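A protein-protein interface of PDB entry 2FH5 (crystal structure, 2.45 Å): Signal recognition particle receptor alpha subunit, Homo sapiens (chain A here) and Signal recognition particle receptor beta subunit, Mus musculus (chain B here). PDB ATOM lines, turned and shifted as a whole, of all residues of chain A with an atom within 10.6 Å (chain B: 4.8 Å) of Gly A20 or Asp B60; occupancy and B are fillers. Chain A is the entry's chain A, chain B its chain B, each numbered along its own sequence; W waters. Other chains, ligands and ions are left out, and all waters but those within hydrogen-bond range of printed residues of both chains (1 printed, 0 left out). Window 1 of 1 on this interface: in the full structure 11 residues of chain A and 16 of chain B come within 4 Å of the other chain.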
ATOM      1  N   ILE A  16      11.417   1.396  16.786  1.00  0.00           N
ATOM      2  CA  ILE A  16      10.999   1.354  18.182  1.00  0.00           C
ATOM      3  C   ILE A  16       9.863   2.353  18.344  1.00  0.00           C
ATOM      4  O   ILE A  16      10.044   3.555  18.063  1.00  0.00           O
ATOM      5  CB  ILE A  16      12.161   1.756  19.150  1.00  0.00           C
ATOM      6  CG1 ILE A  16      13.321   0.745  19.077  1.00  0.00           C
ATOM      7  CG2 ILE A  16      11.649   1.792  20.577  1.00  0.00           C
ATOM      8  CD1 ILE A  16      14.477   1.070  20.067  1.00  0.00           C
ATOM      9  N   PHE A  17       8.693   1.863  18.773  1.00  0.00           N
ATOM     10  CA  PHE A  17       7.543   2.734  18.983  1.00  0.00           C
ATOM     11  C   PHE A  17       6.806   2.414  20.277  1.00  0.00           C
ATOM     12  O   PHE A  17       6.932   1.309  20.812  1.00  0.00           O
ATOM     13  CB  PHE A  17       6.572   2.723  17.770  1.00  0.00           C
ATOM     14  CG  PHE A  17       6.105   1.342  17.323  1.00  0.00           C
ATOM     15  CD1 PHE A  17       6.862   0.585  16.414  1.00  0.00           C
ATOM     16  CD2 PHE A  17       4.889   0.815  17.781  1.00  0.00           C
ATOM     17  CE1 PHE A  17       6.413  -0.681  15.961  1.00  0.00           C
ATOM     18  CE2 PHE A  17       4.431  -0.441  17.340  1.00  0.00           C
ATOM     19  CZ  PHE A  17       5.201  -1.195  16.421  1.00  0.00           C
ATOM     20  N   SER A  18       6.042   3.378  20.797  1.00  0.00           N
ATOM     21  CA  SER A  18       5.319   3.138  22.046  1.00  0.00           C
ATOM     22  C   SER A  18       4.074   2.320  21.740  1.00  0.00           C
ATOM     23  O   SER A  18       3.619   2.279  20.606  1.00  0.00           O
ATOM     24  CB  SER A  18       4.873   4.451  22.684  1.00  0.00           C
ATOM     25  OG  SER A  18       3.802   5.011  21.936  1.00  0.00           O
ATOM     26  N   LYS A  19       3.524   1.657  22.749  1.00  0.00           N
ATOM     27  CA  LYS A  19       2.302   0.895  22.525  1.00  0.00           C
ATOM     28  C   LYS A  19       1.153   1.863  22.186  1.00  0.00           C
ATOM     29  O   LYS A  19       0.135   1.464  21.608  1.00  0.00           O
ATOM     30  CB  LYS A  19       1.966   0.060  23.753  1.00  0.00           C
ATOM     31  CG  LYS A  19       2.834  -1.169  23.861  1.00  0.00           C
ATOM     32  CD  LYS A  19       2.328  -2.065  24.952  1.00  0.00           C
ATOM     33  CE  LYS A  19       3.328  -3.119  25.286  1.00  0.00           C
ATOM     34  NZ  LYS A  19       2.758  -4.068  26.278  1.00  0.00           N
ATOM     35  N   GLY A  20       1.341   3.136  22.534  1.00  0.00           N
ATOM     36  CA  GLY A  20       0.352   4.149  22.225  1.00  0.00           C
ATOM     37  C   GLY A  20       0.326   4.418  20.727  1.00  0.00           C
ATOM     38  O   GLY A  20      -0.615   5.020  20.231  1.00  0.00           O
ATOM     39  N   GLY A  21       1.363   3.961  20.017  1.00  0.00           N
ATOM     40  CA  GLY A  21       1.452   4.138  18.571  1.00  0.00           C
ATOM     41  C   GLY A  21       2.460   5.172  18.083  1.00  0.00           C
ATOM     42  O   GLY A  21       2.580   5.416  16.893  1.00  0.00           O
ATOM     43  N   LEU A  22       3.194   5.783  18.999  1.00  0.00           N
ATOM     44  CA  LEU A  22       4.183   6.777  18.636  1.00  0.00           C
ATOM     45  C   LEU A  22       5.544   6.226  18.202  1.00  0.00           C
ATOM     46  O   LEU A  22       6.235   5.576  18.995  1.00  0.00           O
ATOM     47  CB  LEU A  22       4.382   7.680  19.830  1.00  0.00           C
ATOM     48  CG  LEU A  22       4.055   9.130  19.577  1.00  0.00           C
ATOM     49  CD1 LEU A  22       3.371   9.699  20.837  1.00  0.00           C
ATOM     50  CD2 LEU A  22       5.349   9.856  19.195  1.00  0.00           C
ATOM     51  N   VAL A  23       5.952   6.472  16.964  1.00  0.00           N
ATOM     52  CA  VAL A  23       7.270   5.975  16.536  1.00  0.00           C
ATOM     53  C   VAL A  23       8.316   6.868  17.228  1.00  0.00           C
ATOM     54  O   VAL A  23       8.285   8.086  17.076  1.00  0.00           O
ATOM     55  CB  VAL A  23       7.428   6.044  14.979  1.00  0.00           C
ATOM     56  CG1 VAL A  23       8.818   5.561  14.565  1.00  0.00           C
ATOM     57  CG2 VAL A  23       6.346   5.187  14.306  1.00  0.00           C
ATOM     58  N   LEU A  24       9.227   6.281  17.995  1.00  0.00           N
ATOM     59  CA  LEU A  24      10.244   7.080  18.711  1.00  0.00           C
ATOM     60  C   LEU A  24      11.550   7.124  17.942  1.00  0.00           C
ATOM     61  O   LEU A  24      12.248   8.141  17.938  1.00  0.00           O
ATOM     62  CB  LEU A  24      10.503   6.524  20.127  1.00  0.00           C
ATOM     63  CG  LEU A  24       9.273   6.266  21.023  1.00  0.00           C
ATOM     64  CD1 LEU A  24       9.681   5.673  22.381  1.00  0.00           C
ATOM     65  CD2 LEU A  24       8.517   7.589  21.214  1.00  0.00           C
ATOM     66  N   LEU A  67       8.496  -6.975  23.063  1.00  0.00           N
ATOM     67  CA  LEU A  67       7.820  -5.973  23.869  1.00  0.00           C
ATOM     68  C   LEU A  67       8.487  -5.642  25.181  1.00  0.00           C
ATOM     69  O   LEU A  67       9.208  -6.457  25.761  1.00  0.00           O
ATOM     70  CB  LEU A  67       6.398  -6.409  24.206  1.00  0.00           C
ATOM     71  CG  LEU A  67       5.454  -6.786  23.082  1.00  0.00           C
ATOM     72  CD1 LEU A  67       4.213  -7.381  23.691  1.00  0.00           C
ATOM     73  CD2 LEU A  67       5.143  -5.551  22.231  1.00  0.00           C
ATOM     74  N   ASP A  68       8.229  -4.425  25.637  1.00  0.00           N
ATOM     75  CA  ASP A  68       8.688  -3.969  26.934  1.00  0.00           C
ATOM     76  C   ASP A  68       7.360  -3.564  27.543  1.00  0.00           C
ATOM     77  O   ASP A  68       6.837  -2.482  27.241  1.00  0.00           O
ATOM     78  CB  ASP A  68       9.579  -2.742  26.829  1.00  0.00           C
ATOM     79  CG  ASP A  68      10.093  -2.310  28.180  1.00  0.00           C
ATOM     80  OD1 ASP A  68       9.320  -2.418  29.159  1.00  0.00           O
ATOM     81  OD2 ASP A  68      11.254  -1.859  28.276  1.00  0.00           O
ATOM     82  N   ASN A  69       6.792  -4.425  28.376  1.00  0.00           N
ATOM     83  CA  ASN A  69       5.497  -4.113  28.964  1.00  0.00           C
ATOM     84  C   ASN A  69       5.493  -3.107  30.093  1.00  0.00           C
ATOM     85  O   ASN A  69       4.499  -2.443  30.329  1.00  0.00           O
ATOM     86  CB  ASN A  69       4.816  -5.388  29.401  1.00  0.00           C
ATOM     87  CG  ASN A  69       4.620  -6.328  28.250  1.00  0.00           C
ATOM     88  OD1 ASN A  69       4.186  -5.906  27.177  1.00  0.00           O
ATOM     89  ND2 ASN A  69       4.939  -7.606  28.448  1.00  0.00           N
ATOM     90  N   PHE A  71       7.386  -0.263  30.359  1.00  0.00           N
ATOM     91  CA  PHE A  71       7.368   1.091  29.818  1.00  0.00           C
ATOM     92  C   PHE A  71       6.604   1.243  28.528  1.00  0.00           C
ATOM     93  O   PHE A  71       6.698   2.281  27.901  1.00  0.00           O
ATOM     94  CB  PHE A  71       8.794   1.597  29.610  1.00  0.00           C
ATOM     95  CG  PHE A  71       9.630   1.537  30.854  1.00  0.00           C
ATOM     96  CD1 PHE A  71       9.306   2.322  31.961  1.00  0.00           C
ATOM     97  CD2 PHE A  71      10.711   0.656  30.943  1.00  0.00           C
ATOM     98  CE1 PHE A  71      10.034   2.230  33.141  1.00  0.00           C
ATOM     99  CE2 PHE A  71      11.453   0.553  32.120  1.00  0.00           C
ATOM    100  CZ  PHE A  71      11.110   1.345  33.223  1.00  0.00           C
ATOM    101  N   GLU A  72       5.872   0.201  28.125  1.00  0.00           N
ATOM    102  CA  GLU A  72       5.039   0.226  26.918  1.00  0.00           C
ATOM    103  C   GLU A  72       5.763   0.489  25.601  1.00  0.00           C
ATOM    104  O   GLU A  72       5.441   1.422  24.887  1.00  0.00           O
ATOM    105  CB  GLU A  72       3.912   1.248  27.086  1.00  0.00           C
ATOM    106  CG  GLU A  72       3.127   1.073  28.402  1.00  0.00           C
ATOM    107  CD  GLU A  72       1.748   1.721  28.365  1.00  0.00           C
ATOM    108  OE1 GLU A  72       1.643   2.934  28.071  1.00  0.00           O
ATOM    109  OE2 GLU A  72       0.759   1.001  28.629  1.00  0.00           O
ATOM    110  N   LEU A  73       6.730  -0.362  25.275  1.00  0.00           N
ATOM    111  CA  LEU A  73       7.499  -0.212  24.042  1.00  0.00           C
ATOM    112  C   LEU A  73       7.406  -1.473  23.182  1.00  0.00           C
ATOM    113  O   LEU A  73       7.209  -2.589  23.690  1.00  0.00           O
ATOM    114  CB  LEU A  73       8.968   0.075  24.352  1.00  0.00           C
ATOM    115  CG  LEU A  73       9.347   1.310  25.178  1.00  0.00           C
ATOM    116  CD1 LEU A  73      10.816   1.189  25.522  1.00  0.00           C
ATOM    117  CD2 LEU A  73       9.104   2.604  24.432  1.00  0.00           C
ATOM    118  N   VAL A  74       7.536  -1.264  21.877  1.00  0.00           N
ATOM    119  CA  VAL A  74       7.493  -2.326  20.893  1.00  0.00           C
ATOM    120  C   VAL A  74       8.740  -2.163  20.017  1.00  0.00           C
ATOM    121  O   VAL A  74       9.054  -1.050  19.558  1.00  0.00           O
ATOM    122  CB  VAL A  74       6.243  -2.212  19.982  1.00  0.00           C
ATOM    123  CG1 VAL A  74       6.155  -3.422  19.081  1.00  0.00           C
ATOM    124  CG2 VAL A  74       4.971  -2.048  20.835  1.00  0.00           C
ATOM    125  N   ILE A 107      10.698   7.613  29.099  1.00  0.00           N
ATOM    126  CA  ILE A 107       9.733   6.535  28.983  1.00  0.00           C
ATOM    127  C   ILE A 107       8.975   6.069  30.223  1.00  0.00           C
ATOM    128  O   ILE A 107       7.919   5.457  30.073  1.00  0.00           O
ATOM    129  CB  ILE A 107      10.379   5.268  28.339  1.00  0.00           C
ATOM    130  CG1 ILE A 107      11.396   4.642  29.300  1.00  0.00           C
ATOM    131  CG2 ILE A 107      11.014   5.637  27.034  1.00  0.00           C
ATOM    132  CD1 ILE A 107      12.054   3.353  28.817  1.00  0.00           C
ATOM    133  N   GLN A 109       7.566   7.918  32.508  1.00  0.00           N
ATOM    134  CA  GLN A 109       6.470   8.827  32.771  1.00  0.00           C
ATOM    135  C   GLN A 109       5.187   8.350  32.104  1.00  0.00           C
ATOM    136  O   GLN A 109       5.224   7.616  31.112  1.00  0.00           O
ATOM    137  CB  GLN A 109       6.840  10.229  32.292  1.00  0.00           C
ATOM    138  CG  GLN A 109       7.887  10.880  33.165  1.00  0.00           C
ATOM    139  CD  GLN A 109       8.379  12.173  32.578  1.00  0.00           C
ATOM    140  OE1 GLN A 109       7.584  13.060  32.262  1.00  0.00           O
ATOM    141  NE2 GLN A 109       9.695  12.296  32.419  1.00  0.00           N
ATOM    142  N   GLN A 110       4.055   8.762  32.663  1.00  0.00           N
ATOM    143  CA  GLN A 110       2.757   8.382  32.147  1.00  0.00           C
ATOM    144  C   GLN A 110       2.331   9.267  30.984  1.00  0.00           C
ATOM    145  O   GLN A 110       1.817   8.788  29.980  1.00  0.00           O
ATOM    146  CB  GLN A 110       1.729   8.465  33.275  1.00  0.00           C
ATOM    147  CG  GLN A 110       0.266   8.540  32.839  1.00  0.00           C
ATOM    148  CD  GLN A 110      -0.231   7.245  32.224  1.00  0.00           C
ATOM    149  OE1 GLN A 110      -0.010   6.157  32.772  1.00  0.00           O
ATOM    150  NE2 GLN A 110      -0.921   7.355  31.089  1.00  0.00           N
ATOM    151  N   SER A 111       2.544  10.564  31.116  1.00  0.00           N
ATOM    152  CA  SER A 111       2.134  11.492  30.085  1.00  0.00           C
ATOM    153  C   SER A 111       2.823  11.220  28.747  1.00  0.00           C
ATOM    154  O   SER A 111       4.023  10.966  28.699  1.00  0.00           O
ATOM    155  CB  SER A 111       2.426  12.919  30.545  1.00  0.00           C
ATOM    156  OG  SER A 111       2.111  13.873  29.529  1.00  0.00           O
ATOM    157  N   ALA A 112       2.064  11.278  27.659  1.00  0.00           N
ATOM    158  CA  ALA A 112       2.630  11.073  26.330  1.00  0.00           C
ATOM    159  C   ALA A 112       3.556  12.245  25.970  1.00  0.00           C
ATOM    160  O   ALA A 112       4.459  12.101  25.139  1.00  0.00           O
ATOM    161  CB  ALA A 112       1.520  10.958  25.303  1.00  0.00           C
ATOM    162  N   LEU A 113       3.323  13.410  26.579  1.00  0.00           N
ATOM    163  CA  LEU A 113       4.164  14.585  26.310  1.00  0.00           C
ATOM    164  C   LEU A 113       5.630  14.218  26.574  1.00  0.00           C
ATOM    165  O   LEU A 113       6.550  14.706  25.922  1.00  0.00           O
ATOM    166  CB  LEU A 113       3.751  15.765  27.208  1.00  0.00           C
ATOM    167  CG  LEU A 113       2.513  16.565  26.793  1.00  0.00           C
ATOM    168  CD1 LEU A 113       2.209  17.579  27.856  1.00  0.00           C
ATOM    169  CD2 LEU A 113       2.742  17.242  25.439  1.00  0.00           C
ATOM    170  N   LEU A 115       7.139  11.529  25.812  1.00  0.00           N
ATOM    171  CA  LEU A 115       7.730  10.861  24.643  1.00  0.00           C
ATOM    172  C   LEU A 115       7.749  11.867  23.518  1.00  0.00           C
ATOM    173  O   LEU A 115       8.673  11.907  22.694  1.00  0.00           O
ATOM    174  CB  LEU A 115       6.903   9.633  24.205  1.00  0.00           C
ATOM    175  CG  LEU A 115       6.670   8.531  25.242  1.00  0.00           C
ATOM    176  CD1 LEU A 115       5.681   7.498  24.719  1.00  0.00           C
ATOM    177  CD2 LEU A 115       7.972   7.859  25.588  1.00  0.00           C
ATOM    178  N   LEU A 116       6.699  12.679  23.478  1.00  0.00           N
ATOM    179  CA  LEU A 116       6.567  13.688  22.439  1.00  0.00           C
ATOM    180  C   LEU A 116       7.644  14.759  22.532  1.00  0.00           C
ATOM    181  O   LEU A 116       8.086  15.274  21.509  1.00  0.00           O
ATOM    182  CB  LEU A 116       5.175  14.329  22.485  1.00  0.00           C
ATOM    183  CG  LEU A 116       3.980  13.456  22.101  1.00  0.00           C
ATOM    184  CD1 LEU A 116       2.696  14.151  22.442  1.00  0.00           C
ATOM    185  CD2 LEU A 116       4.031  13.136  20.620  1.00  0.00           C
ATOM    186  N   PHE B  12     -10.792  10.224  22.586  1.00  0.00           N
ATOM    187  CA  PHE B  12     -10.747  10.201  21.125  1.00  0.00           C
ATOM    188  C   PHE B  12     -10.963   8.724  20.758  1.00  0.00           C
ATOM    189  O   PHE B  12     -10.201   7.844  21.190  1.00  0.00           O
ATOM    190  CB  PHE B  12      -9.392  10.681  20.610  1.00  0.00           C
ATOM    191  CG  PHE B  12      -9.182  12.161  20.743  1.00  0.00           C
ATOM    192  CD1 PHE B  12      -8.977  12.744  21.989  1.00  0.00           C
ATOM    193  CD2 PHE B  12      -9.241  12.986  19.627  1.00  0.00           C
ATOM    194  CE1 PHE B  12      -8.838  14.134  22.122  1.00  0.00           C
ATOM    195  CE2 PHE B  12      -9.102  14.373  19.755  1.00  0.00           C
ATOM    196  CZ  PHE B  12      -8.899  14.943  21.011  1.00  0.00           C
ATOM    197  N   LYS B  20      -6.752   9.177  15.132  1.00  0.00           N
ATOM    198  CA  LYS B  20      -6.831   9.582  16.535  1.00  0.00           C
ATOM    199  C   LYS B  20      -5.494   9.969  17.118  1.00  0.00           C
ATOM    200  O   LYS B  20      -5.374  11.018  17.741  1.00  0.00           O
ATOM    201  CB  LYS B  20      -7.470   8.475  17.409  1.00  0.00           C
ATOM    202  CG  LYS B  20      -8.923   8.114  17.024  1.00  0.00           C
ATOM    203  CD  LYS B  20      -9.457   6.886  17.808  1.00  0.00           C
ATOM    204  CE  LYS B  20      -8.647   5.613  17.552  1.00  0.00           C
ATOM    205  NZ  LYS B  20      -8.642   5.185  16.127  1.00  0.00           N
ATOM    206  N   THR B  21      -4.477   9.139  16.899  1.00  0.00           N
ATOM    207  CA  THR B  21      -3.181   9.438  17.459  1.00  0.00           C
ATOM    208  C   THR B  21      -2.526  10.651  16.834  1.00  0.00           C
ATOM    209  O   THR B  21      -1.903  11.421  17.552  1.00  0.00           O
ATOM    210  CB  THR B  21      -2.256   8.229  17.367  1.00  0.00           C
ATOM    211  OG1 THR B  21      -2.872   7.155  18.066  1.00  0.00           O
ATOM    212  CG2 THR B  21      -0.918   8.506  18.062  1.00  0.00           C
ATOM    213  N   PHE B  24      -4.158  13.734  18.229  1.00  0.00           N
ATOM    214  CA  PHE B  24      -3.689  13.807  19.603  1.00  0.00           C
ATOM    215  C   PHE B  24      -2.312  14.498  19.619  1.00  0.00           C
ATOM    216  O   PHE B  24      -2.081  15.413  20.412  1.00  0.00           O
ATOM    217  CB  PHE B  24      -3.629  12.367  20.140  1.00  0.00           C
ATOM    218  CG  PHE B  24      -3.080  12.213  21.529  1.00  0.00           C
ATOM    219  CD1 PHE B  24      -3.862  12.472  22.640  1.00  0.00           C
ATOM    220  CD2 PHE B  24      -1.813  11.670  21.726  1.00  0.00           C
ATOM    221  CE1 PHE B  24      -3.396  12.178  23.948  1.00  0.00           C
ATOM    222  CE2 PHE B  24      -1.335  11.374  23.026  1.00  0.00           C
ATOM    223  CZ  PHE B  24      -2.130  11.624  24.128  1.00  0.00           C
ATOM    224  N   SER B  38      -2.143   1.654  17.334  1.00  0.00           N
ATOM    225  CA  SER B  38      -2.070   1.731  18.792  1.00  0.00           C
ATOM    226  C   SER B  38      -2.569   0.476  19.475  1.00  0.00           C
ATOM    227  O   SER B  38      -3.598  -0.061  19.081  1.00  0.00           O
ATOM    228  CB  SER B  38      -2.909   2.915  19.290  1.00  0.00           C
ATOM    229  OG  SER B  38      -2.352   4.141  18.864  1.00  0.00           O
ATOM    230  N   THR B  40      -2.522   0.290  23.180  1.00  0.00           N
ATOM    231  CA  THR B  40      -3.018   0.720  24.500  1.00  0.00           C
ATOM    232  C   THR B  40      -3.391   2.190  24.360  1.00  0.00           C
ATOM    233  O   THR B  40      -3.096   2.836  23.358  1.00  0.00           O
ATOM    234  CB  THR B  40      -2.008   0.668  25.697  1.00  0.00           C
ATOM    235  OG1 THR B  40      -0.806   1.369  25.360  1.00  0.00           O
ATOM    236  CG2 THR B  40      -1.715  -0.743  26.105  1.00  0.00           C
ATOM    237  N   ASP B  41      -4.024   2.712  25.389  1.00  0.00           N
ATOM    238  CA  ASP B  41      -4.414   4.106  25.411  1.00  0.00           C
ATOM    239  C   ASP B  41      -3.204   4.946  25.796  1.00  0.00           C
ATOM    240  O   ASP B  41      -2.249   4.448  26.369  1.00  0.00           O
ATOM    241  CB  ASP B  41      -5.468   4.299  26.480  1.00  0.00           C
ATOM    242  CG  ASP B  41      -4.999   3.769  27.827  1.00  0.00           C
ATOM    243  OD1 ASP B  41      -5.010   2.531  28.028  1.00  0.00           O
ATOM    244  OD2 ASP B  41      -4.590   4.584  28.685  1.00  0.00           O
ATOM    245  N   SER B  42      -3.253   6.223  25.458  1.00  0.00           N
ATOM    246  CA  SER B  42      -2.222   7.158  25.850  1.00  0.00           C
ATOM    247  C   SER B  42      -2.951   8.450  26.272  1.00  0.00           C
ATOM    248  O   SER B  42      -4.043   8.777  25.792  1.00  0.00           O
ATOM    249  CB  SER B  42      -1.179   7.380  24.725  1.00  0.00           C
ATOM    250  OG  SER B  42      -1.725   7.621  23.446  1.00  0.00           O
ATOM    251  N   LEU B  58      -6.477  14.765  27.526  1.00  0.00           N
ATOM    252  CA  LEU B  58      -6.787  14.064  26.287  1.00  0.00           C
ATOM    253  C   LEU B  58      -6.390  12.603  26.480  1.00  0.00           C
ATOM    254  O   LEU B  58      -5.312  12.317  27.016  1.00  0.00           O
ATOM    255  CB  LEU B  58      -6.003  14.657  25.116  1.00  0.00           C
ATOM    256  CG  LEU B  58      -6.017  16.179  24.931  1.00  0.00           C
ATOM    257  CD1 LEU B  58      -5.358  16.528  23.610  1.00  0.00           C
ATOM    258  CD2 LEU B  58      -7.444  16.716  24.935  1.00  0.00           C
ATOM    259  N   ILE B  59      -7.280  11.693  26.082  1.00  0.00           N
ATOM    260  CA  ILE B  59      -7.042  10.253  26.158  1.00  0.00           C
ATOM    261  C   ILE B  59      -7.318   9.651  24.777  1.00  0.00           C
ATOM    262  O   ILE B  59      -8.452   9.680  24.286  1.00  0.00           O
ATOM    263  CB  ILE B  59      -7.962   9.572  27.165  1.00  0.00           C
ATOM    264  CG1 ILE B  59      -7.693  10.106  28.571  1.00  0.00           C
ATOM    265  CG2 ILE B  59      -7.765   8.077  27.119  1.00  0.00           C
ATOM    266  CD1 ILE B  59      -8.581   9.440  29.633  1.00  0.00           C
ATOM    267  N   ASP B  60      -6.267   9.129  24.150  1.00  0.00           N
ATOM    268  CA  ASP B  60      -6.332   8.528  22.819  1.00  0.00           C
ATOM    269  C   ASP B  60      -6.637   7.050  22.979  1.00  0.00           C
ATOM    270  O   ASP B  60      -5.832   6.342  23.539  1.00  0.00           O
ATOM    271  CB  ASP B  60      -4.969   8.757  22.131  1.00  0.00           C
ATOM    272  CG  ASP B  60      -4.766   7.927  20.838  1.00  0.00           C
ATOM    273  OD1 ASP B  60      -5.732   7.705  20.080  1.00  0.00           O
ATOM    274  OD2 ASP B  60      -3.601   7.510  20.570  1.00  0.00           O
ATOM    275  N   LEU B  61      -7.779   6.576  22.489  1.00  0.00           N
ATOM    276  CA  LEU B  61      -8.133   5.144  22.636  1.00  0.00           C
ATOM    277  C   LEU B  61      -7.953   4.321  21.361  1.00  0.00           C
ATOM    278  O   LEU B  61      -8.374   4.718  20.294  1.00  0.00           O
ATOM    279  CB  LEU B  61      -9.581   4.976  23.147  1.00  0.00           C
ATOM    280  CG  LEU B  61      -9.952   5.620  24.505  1.00  0.00           C
ATOM    281  CD1 LEU B  61     -11.385   5.283  24.898  1.00  0.00           C
ATOM    282  CD2 LEU B  61      -9.003   5.122  25.589  1.00  0.00           C
ATOM    283  N   PRO B  62      -7.315   3.146  21.468  1.00  0.00           N
ATOM    284  CA  PRO B  62      -7.093   2.282  20.307  1.00  0.00           C
ATOM    285  C   PRO B  62      -8.397   1.967  19.565  1.00  0.00           C
ATOM    286  O   PRO B  62      -9.416   1.686  20.184  1.00  0.00           O
ATOM    287  CB  PRO B  62      -6.492   1.019  20.923  1.00  0.00           C
ATOM    288  CG  PRO B  62      -5.920   1.459  22.197  1.00  0.00           C
ATOM    289  CD  PRO B  62      -6.916   2.464  22.708  1.00  0.00           C
HETATM  290  O   HOH W   1      -2.447   6.049  29.149  1.00  0.00           O
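Among the printed residues, pairs that only touch across the chains: Lys A19 with Ser B38 (3.6 Å), Gly A20 with Thr B21 (3.8 Å), Gly A20 with Thr B40 (3.9 Å), Gly A20 with Asp B60 (3.9 Å), Gly A21 with Ser B38 (3.8 Å), Glu A72 with Thr B40 (3.6 Å) and Ala A112 with Phe B24 (3.7 Å).
OG of Ser A18 lies close to N of Gly A20 (3.2 Å). The side-chain hydroxyl of Ser A18 sits at hydrogen-bond distance from the backbone NH of Gly A21, at 3.3 Å. The side-chain amide oxygen (OD1) of Asn A69 is in hydrogen-bond range of the side-chain amino group (NZ) of Lys A19 (2.5 Å). The backbone carbonyl oxygen (O) of Glu A72 is in hydrogen-bond range of the backbone NH (N) of Lys A19, at 2.9 Å. The side-chain hydroxyl (OG1) of Thr B21 sits close to the side-chain carboxylate (OD2) of Asp B60 (2.6 Å). The backbone NH of Asp B60 sits at hydrogen-bond distance from the backbone carbonyl oxygen of Ser B42.
Of the printed residues of chain B, Lys A19 touches Ser B38 and Thr B40. Of the printed residues of chain B, Gly A21 touches Ser B38. Of the printed residues of chain B, Glu A72 touches Thr B40 (3.6 Å). Of the printed residues of chain B, Ala A112 touches Phe B24 (3.7 Å). No residue of chain A comes within 4 Å of Lys B20. Thr B21 touches one residue of chain A. Of the printed residues of chain A, Phe B24 touches Ala A112. Ser B38 touches just these residues of chain A: Lys A19, Gly A20 and Gly A21. Thr B40 touches just these residues of chain A: Lys A19, Gly A20 and Glu A72. Asp B60 touches just one residue of chain A: Gly A20. No residue of chain A comes within 4 Å of Leu B61.
Of the 24 printed residues of chain A, 5 touch a printed residue of chain B. Of the 13 printed residues of chain B, 5 touch a printed residue of chain A. Printed residues of chain B that touch a printed residue of chain A: Thr B21, Phe B24, Ser B38, Thr B40 and Asp B60. Hydrophobic or aromatic side chains of chain B that line the printed part of chain A: Phe B24. Among the printed residues, no Asp or Glu carboxylate lies within 4 Å of a Lys or Arg side-chain nitrogen of the other chain.
Water W1 bridges OD2 of Asp B41 and NE2 of Gln A110.
The backbone NH of Thr B40 is in hydrogen-bond range of the backbone carbonyl oxygen of Lys A19 (3.3 Å). O of Gly A20 sits close to OG of Ser B38 (2.4 Å).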
